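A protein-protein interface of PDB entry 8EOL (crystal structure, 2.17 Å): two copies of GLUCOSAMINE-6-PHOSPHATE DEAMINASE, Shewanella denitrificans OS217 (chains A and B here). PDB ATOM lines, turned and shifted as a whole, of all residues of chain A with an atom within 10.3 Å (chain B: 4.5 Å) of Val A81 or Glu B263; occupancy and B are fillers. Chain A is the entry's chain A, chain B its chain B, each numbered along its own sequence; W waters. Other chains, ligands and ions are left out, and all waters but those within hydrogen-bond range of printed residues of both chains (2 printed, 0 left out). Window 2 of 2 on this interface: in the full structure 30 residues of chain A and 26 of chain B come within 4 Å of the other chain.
OD2 of Asp B262 is in hydrogen-bond range of OH of Tyr A82 (2.6 Å).
The backbone NH of Tyr A82 lies within hydrogen-bond range of the backbone carbonyl oxygen of Ser A77, 2.9 Å away.
The guanidinium group (NH1) of Arg B211 sits at hydrogen-bond distance from the side-chain hydroxyl (OG) of Ser B267.
The side-chain hydroxyl (OG) of Ser B264 sits at hydrogen-bond distance from the side-chain carboxylate (OD1) of Asp B262, 2.5 Å away.
OE2 of Glu B263 is in salt-bridge range of NH2 of Arg B295, 2.9 Å away.
Among the printed residues, pairs that only touch across the chains: Ser A77 with Arg B211 (3.6 Å), Val A81 with Arg B211 (3.5 Å), Val A81 with Glu B263 (3.4 Å), Val A81 with Ser B264 (3.3 Å), Tyr A82 with Arg B211 (3.9 Å), Tyr A82 with Glu B263 (3.4 Å) and Tyr A82 with Ser B264 (3.6 Å).
Of chain B, only Arg B211, Glu B263 and Ser B264 come within 4 Å of Val A81.
Glu B263 touches just these residues of chain A: Val A81 (3.4 Å) and Tyr A82 (3.4 Å).
Asp B262 touches just one residue of chain A: Tyr A82 (2.6 Å).
Printed residues of chain B within 4 Å of Tyr A82: Arg B211 (3.9 Å), Asp B262 (2.6 Å), Glu B263 (3.4 Å) and Ser B264 (3.6 Å).
Printed residues of chain B within 4 Å of Ser A77: Arg B211 (3.6 Å).
Val A78 touches none of the printed residues of chain B.
The nearest residue of chain B that does not touch Val A81 is Ser B267 (4.4 Å).
Of the 16 printed residues of chain A, 3 touch a printed residue of chain B.
Hydrophobic or aromatic side chains of chain A that line the printed part of chain B: Val A81 and Tyr A82.
Of the 7 printed residues of chain B, 4 touch a printed residue of chain A.
No position is printed for both chains.
Of the 8 pairs that touch across the chains among the printed residues, none has its exchanged pair printed and touching as well.
Water W1 lies within hydrogen-bond range of O of Arg B211, OD2 of Asp B262, OH of Tyr A82 and OG of Ser B264.
Water W2 lies within hydrogen-bond range of NH2 of Arg B295 (2.8 Å) and NZ of Lys A84 (3.2 Å).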
ATOM      1  N   ALA A  75      17.763  -6.811 -15.086  1.00  0.00           N
ATOM      2  CA  ALA A  75      17.380  -8.065 -15.730  1.00  0.00           C
ATOM      3  C   ALA A  75      16.361  -8.724 -14.809  1.00  0.00           C
ATOM      4  O   ALA A  75      16.723  -9.115 -13.681  1.00  0.00           O
ATOM      5  CB  ALA A  75      18.589  -8.984 -15.966  1.00  0.00           C
ATOM      6  N   PRO A  76      15.075  -8.786 -15.188  1.00  0.00           N
ATOM      7  CA  PRO A  76      14.044  -9.246 -14.235  1.00  0.00           C
ATOM      8  C   PRO A  76      14.309 -10.613 -13.619  1.00  0.00           C
ATOM      9  O   PRO A  76      13.992 -10.813 -12.436  1.00  0.00           O
ATOM     10  CB  PRO A  76      12.758  -9.261 -15.083  1.00  0.00           C
ATOM     11  CG  PRO A  76      13.013  -8.357 -16.201  1.00  0.00           C
ATOM     12  CD  PRO A  76      14.495  -8.458 -16.500  1.00  0.00           C
ATOM     13  N   SER A  77      14.922 -11.549 -14.354  1.00  0.00           N
ATOM     14  CA  SER A  77      15.060 -12.891 -13.805  1.00  0.00           C
ATOM     15  C   SER A  77      16.047 -12.955 -12.653  1.00  0.00           C
ATOM     16  O   SER A  77      16.016 -13.924 -11.888  1.00  0.00           O
ATOM     17  CB  SER A  77      15.480 -13.878 -14.905  1.00  0.00           C
ATOM     18  OG  SER A  77      16.772 -13.572 -15.381  1.00  0.00           O
ATOM     19  N   VAL A  78      16.946 -11.977 -12.525  1.00  0.00           N
ATOM     20  CA  VAL A  78      17.891 -12.010 -11.412  1.00  0.00           C
ATOM     21  C   VAL A  78      17.125 -11.936 -10.094  1.00  0.00           C
ATOM     22  O   VAL A  78      17.395 -12.685  -9.142  1.00  0.00           O
ATOM     23  CB  VAL A  78      18.936 -10.875 -11.543  1.00  0.00           C
ATOM     24  CG1 VAL A  78      19.747 -10.730 -10.249  1.00  0.00           C
ATOM     25  CG2 VAL A  78      19.870 -11.102 -12.751  1.00  0.00           C
ATOM     26  N   ALA A  79      16.111 -11.070 -10.048  1.00  0.00           N
ATOM     27  CA  ALA A  79      15.276 -10.961  -8.867  1.00  0.00           C
ATOM     28  C   ALA A  79      14.294 -12.121  -8.788  1.00  0.00           C
ATOM     29  O   ALA A  79      14.195 -12.780  -7.748  1.00  0.00           O
ATOM     30  CB  ALA A  79      14.555  -9.614  -8.869  1.00  0.00           C
ATOM     31  N   SER A  80      13.553 -12.393  -9.874  1.00  0.00           N
ATOM     32  CA  SER A  80      12.394 -13.285  -9.749  1.00  0.00           C
ATOM     33  C   SER A  80      12.768 -14.765  -9.799  1.00  0.00           C
ATOM     34  O   SER A  80      12.225 -15.565  -9.030  1.00  0.00           O
ATOM     35  CB  SER A  80      11.333 -12.943 -10.811  1.00  0.00           C
ATOM     36  OG  SER A  80      11.799 -13.045 -12.144  1.00  0.00           O
ATOM     37  N   VAL A  81      13.675 -15.153 -10.686  1.00  0.00           N
ATOM     38  CA  VAL A  81      14.024 -16.563 -10.860  1.00  0.00           C
ATOM     39  C   VAL A  81      15.228 -16.968 -10.017  1.00  0.00           C
ATOM     40  O   VAL A  81      15.241 -18.027  -9.380  1.00  0.00           O
ATOM     41  CB  VAL A  81      14.285 -16.838 -12.350  1.00  0.00           C
ATOM     42  CG1 VAL A  81      14.959 -18.150 -12.481  1.00  0.00           C
ATOM     43  CG2 VAL A  81      12.973 -16.852 -13.110  1.00  0.00           C
ATOM     44  N   TYR A  82      16.303 -16.182 -10.066  1.00  0.00           N
ATOM     45  CA  TYR A  82      17.472 -16.515  -9.270  1.00  0.00           C
ATOM     46  C   TYR A  82      17.319 -16.041  -7.832  1.00  0.00           C
ATOM     47  O   TYR A  82      18.124 -16.417  -6.983  1.00  0.00           O
ATOM     48  CB  TYR A  82      18.724 -15.922  -9.942  1.00  0.00           C
ATOM     49  CG  TYR A  82      19.042 -16.606 -11.276  1.00  0.00           C
ATOM     50  CD1 TYR A  82      19.781 -17.794 -11.303  1.00  0.00           C
ATOM     51  CD2 TYR A  82      18.574 -16.093 -12.481  1.00  0.00           C
ATOM     52  CE1 TYR A  82      20.052 -18.459 -12.497  1.00  0.00           C
ATOM     53  CE2 TYR A  82      18.838 -16.736 -13.675  1.00  0.00           C
ATOM     54  CZ  TYR A  82      19.582 -17.917 -13.676  1.00  0.00           C
ATOM     55  OH  TYR A  82      19.837 -18.534 -14.864  1.00  0.00           O
ATOM     56  N   GLY A  83      16.316 -15.214  -7.556  1.00  0.00           N
ATOM     57  CA  GLY A  83      16.033 -14.798  -6.194  1.00  0.00           C
ATOM     58  C   GLY A  83      17.110 -13.965  -5.536  1.00  0.00           C
ATOM     59  O   GLY A  83      17.312 -14.090  -4.330  1.00  0.00           O
ATOM     60  N   LYS A  84      17.770 -13.069  -6.273  1.00  0.00           N
ATOM     61  CA  LYS A  84      18.913 -12.339  -5.729  1.00  0.00           C
ATOM     62  C   LYS A  84      18.558 -10.877  -5.502  1.00  0.00           C
ATOM     63  O   LYS A  84      17.841 -10.253  -6.291  1.00  0.00           O
ATOM     64  CB  LYS A  84      20.148 -12.443  -6.642  1.00  0.00           C
ATOM     65  CG  LYS A  84      20.611 -13.867  -6.890  1.00  0.00           C
ATOM     66  CD  LYS A  84      21.231 -14.561  -5.648  1.00  0.00           C
ATOM     67  CE  LYS A  84      21.342 -16.091  -5.914  1.00  0.00           C
ATOM     68  NZ  LYS A  84      22.412 -16.833  -5.169  1.00  0.00           N
ATOM     69  N   THR A  85      19.013 -10.354  -4.385  1.00  0.00           N
ATOM     70  CA  THR A  85      18.978  -8.924  -4.128  1.00  0.00           C
ATOM     71  C   THR A  85      20.322  -8.338  -4.532  1.00  0.00           C
ATOM     72  O   THR A  85      21.367  -8.975  -4.364  1.00  0.00           O
ATOM     73  CB  THR A  85      18.700  -8.649  -2.658  1.00  0.00           C
ATOM     74  OG1 THR A  85      19.784  -9.193  -1.880  1.00  0.00           O
ATOM     75  CG2 THR A  85      17.345  -9.300  -2.244  1.00  0.00           C
ATOM     76  N   PRO A 103       3.367  -9.247 -10.703  1.00  0.00           N
ATOM     77  CA  PRO A 103       4.151  -9.740  -9.558  1.00  0.00           C
ATOM     78  C   PRO A 103       5.631  -9.474  -9.697  1.00  0.00           C
ATOM     79  O   PRO A 103       6.283  -9.069  -8.722  1.00  0.00           O
ATOM     80  CB  PRO A 103       3.877 -11.258  -9.563  1.00  0.00           C
ATOM     81  CG  PRO A 103       2.768 -11.479 -10.541  1.00  0.00           C
ATOM     82  CD  PRO A 103       2.836 -10.356 -11.520  1.00  0.00           C
ATOM     83  N   ASP A 104       6.180  -9.725 -10.891  1.00  0.00           N
ATOM     84  CA  ASP A 104       7.604  -9.517 -11.125  1.00  0.00           C
ATOM     85  C   ASP A 104       7.999  -8.055 -10.926  1.00  0.00           C
ATOM     86  O   ASP A 104       9.040  -7.771 -10.340  1.00  0.00           O
ATOM     87  CB  ASP A 104       7.970 -10.016 -12.516  1.00  0.00           C
ATOM     88  CG  ASP A 104       8.077 -11.540 -12.569  1.00  0.00           C
ATOM     89  OD1 ASP A 104       7.511 -12.218 -11.664  1.00  0.00           O
ATOM     90  OD2 ASP A 104       8.755 -12.055 -13.493  1.00  0.00           O
ATOM     91  N   ALA A 107       7.849  -7.433  -7.183  1.00  0.00           N
ATOM     92  CA  ALA A 107       8.978  -8.115  -6.553  1.00  0.00           C
ATOM     93  C   ALA A 107      10.286  -7.350  -6.753  1.00  0.00           C
ATOM     94  O   ALA A 107      11.086  -7.217  -5.815  1.00  0.00           O
ATOM     95  CB  ALA A 107       9.112  -9.528  -7.116  1.00  0.00           C
ATOM     96  N   GLN A 108      10.542  -6.866  -7.980  1.00  0.00           N
ATOM     97  CA  GLN A 108      11.746  -6.069  -8.217  1.00  0.00           C
ATOM     98  C   GLN A 108      11.721  -4.790  -7.394  1.00  0.00           C
ATOM     99  O   GLN A 108      12.755  -4.347  -6.875  1.00  0.00           O
ATOM    100  CB  GLN A 108      11.851  -5.741  -9.698  1.00  0.00           C
ATOM    101  CG  GLN A 108      12.230  -6.939 -10.547  1.00  0.00           C
ATOM    102  CD  GLN A 108      12.368  -6.575 -12.013  1.00  0.00           C
ATOM    103  OE1 GLN A 108      13.416  -6.139 -12.454  1.00  0.00           O
ATOM    104  NE2 GLN A 108      11.276  -6.725 -12.767  1.00  0.00           N
ATOM    105  N   MET A 111      12.493  -5.518  -3.630  1.00  0.00           N
ATOM    106  CA  MET A 111      13.902  -5.840  -3.493  1.00  0.00           C
ATOM    107  C   MET A 111      14.755  -4.597  -3.622  1.00  0.00           C
ATOM    108  O   MET A 111      15.716  -4.419  -2.860  1.00  0.00           O
ATOM    109  CB  MET A 111      14.277  -6.879  -4.535  1.00  0.00           C
ATOM    110  CG  MET A 111      13.696  -8.203  -4.119  1.00  0.00           C
ATOM    111  SD  MET A 111      13.403  -9.428  -5.386  1.00  0.00           S
ATOM    112  CE  MET A 111      11.960 -10.179  -4.618  1.00  0.00           C
ATOM    113  N   ARG B 211      16.760 -18.604 -20.695  1.00  0.00           N
ATOM    114  CA  ARG B 211      16.435 -17.813 -19.519  1.00  0.00           C
ATOM    115  C   ARG B 211      17.709 -17.606 -18.710  1.00  0.00           C
ATOM    116  O   ARG B 211      18.487 -18.552 -18.530  1.00  0.00           O
ATOM    117  CB  ARG B 211      15.373 -18.509 -18.668  1.00  0.00           C
ATOM    118  CG  ARG B 211      14.717 -17.585 -17.706  1.00  0.00           C
ATOM    119  CD  ARG B 211      13.689 -16.735 -18.420  1.00  0.00           C
ATOM    120  NE  ARG B 211      13.277 -15.671 -17.515  1.00  0.00           N
ATOM    121  CZ  ARG B 211      12.346 -15.776 -16.567  1.00  0.00           C
ATOM    122  NH1 ARG B 211      11.666 -16.917 -16.396  1.00  0.00           N
ATOM    123  NH2 ARG B 211      12.109 -14.720 -15.788  1.00  0.00           N
ATOM    124  N   ASP B 262      19.580 -24.746 -14.149  1.00  0.00           N
ATOM    125  CA  ASP B 262      19.845 -23.956 -12.951  1.00  0.00           C
ATOM    126  C   ASP B 262      18.536 -23.452 -12.353  1.00  0.00           C
ATOM    127  O   ASP B 262      17.462 -23.984 -12.651  1.00  0.00           O
ATOM    128  CB  ASP B 262      20.795 -22.798 -13.272  1.00  0.00           C
ATOM    129  CG  ASP B 262      20.208 -21.791 -14.281  1.00  0.00           C
ATOM    130  OD1 ASP B 262      19.067 -21.995 -14.752  1.00  0.00           O
ATOM    131  OD2 ASP B 262      20.932 -20.828 -14.639  1.00  0.00           O
ATOM    132  N   GLU B 263      18.606 -22.410 -11.541  1.00  0.00           N
ATOM    133  CA  GLU B 263      17.388 -21.879 -10.932  1.00  0.00           C
ATOM    134  C   GLU B 263      16.310 -21.523 -11.967  1.00  0.00           C
ATOM    135  O   GLU B 263      15.124 -21.479 -11.629  1.00  0.00           O
ATOM    136  CB  GLU B 263      17.720 -20.641 -10.105  1.00  0.00           C
ATOM    137  CG  GLU B 263      18.673 -20.896  -8.887  1.00  0.00           C
ATOM    138  CD  GLU B 263      20.162 -20.695  -9.254  1.00  0.00           C
ATOM    139  OE1 GLU B 263      20.563 -21.060 -10.388  1.00  0.00           O
ATOM    140  OE2 GLU B 263      20.925 -20.147  -8.428  1.00  0.00           O
ATOM    141  N   SER B 264      16.687 -21.269 -13.215  1.00  0.00           N
ATOM    142  CA  SER B 264      15.693 -20.883 -14.204  1.00  0.00           C
ATOM    143  C   SER B 264      14.985 -22.058 -14.851  1.00  0.00           C
ATOM    144  O   SER B 264      14.082 -21.823 -15.648  1.00  0.00           O
ATOM    145  CB  SER B 264      16.345 -20.029 -15.282  1.00  0.00           C
ATOM    146  OG  SER B 264      17.231 -20.802 -16.029  1.00  0.00           O
ATOM    147  N   TYR B 265      15.361 -23.293 -14.512  1.00  0.00           N
ATOM    148  CA  TYR B 265      14.854 -24.482 -15.196  1.00  0.00           C
ATOM    149  C   TYR B 265      13.332 -24.547 -15.179  1.00  0.00           C
ATOM    150  O   TYR B 265      12.693 -24.668 -16.230  1.00  0.00           O
ATOM    151  CB  TYR B 265      15.425 -25.738 -14.533  1.00  0.00           C
ATOM    152  CG  TYR B 265      14.963 -27.036 -15.159  1.00  0.00           C
ATOM    153  CD1 TYR B 265      15.620 -27.554 -16.277  1.00  0.00           C
ATOM    154  CD2 TYR B 265      13.881 -27.756 -14.634  1.00  0.00           C
ATOM    155  CE1 TYR B 265      15.214 -28.735 -16.869  1.00  0.00           C
ATOM    156  CE2 TYR B 265      13.474 -28.961 -15.217  1.00  0.00           C
ATOM    157  CZ  TYR B 265      14.150 -29.437 -16.333  1.00  0.00           C
ATOM    158  OH  TYR B 265      13.790 -30.610 -16.938  1.00  0.00           O
ATOM    159  N   SER B 267      10.853 -22.439 -14.562  1.00  0.00           N
ATOM    160  CA  SER B 267      10.123 -21.431 -15.321  1.00  0.00           C
ATOM    161  C   SER B 267      10.368 -21.569 -16.820  1.00  0.00           C
ATOM    162  O   SER B 267       9.442 -21.388 -17.622  1.00  0.00           O
ATOM    163  CB  SER B 267      10.514 -20.037 -14.842  1.00  0.00           C
ATOM    164  OG  SER B 267       9.941 -19.051 -15.687  1.00  0.00           O
ATOM    165  N   ARG B 295      26.453 -23.305 -13.105  1.00  0.00           N
ATOM    166  CA  ARG B 295      27.071 -22.100 -13.648  1.00  0.00           C
ATOM    167  C   ARG B 295      28.015 -22.381 -14.800  1.00  0.00           C
ATOM    168  O   ARG B 295      28.369 -21.452 -15.531  1.00  0.00           O
ATOM    169  CB  ARG B 295      27.819 -21.351 -12.553  1.00  0.00           C
ATOM    170  CG  ARG B 295      26.946 -20.827 -11.436  1.00  0.00           C
ATOM    171  CD  ARG B 295      26.190 -19.553 -11.822  1.00  0.00           C
ATOM    172  NE  ARG B 295      25.417 -19.150 -10.647  1.00  0.00           N
ATOM    173  CZ  ARG B 295      24.154 -19.515 -10.413  1.00  0.00           C
ATOM    174  NH1 ARG B 295      23.490 -20.261 -11.301  1.00  0.00           N
ATOM    175  NH2 ARG B 295      23.555 -19.152  -9.273  1.00  0.00           N
HETATM  176  O   HOH W   1      20.227 -20.198 -17.420  1.00  0.00           O
HETATM  177  O   HOH W   2      24.728 -18.238  -6.858  1.00  0.00           O
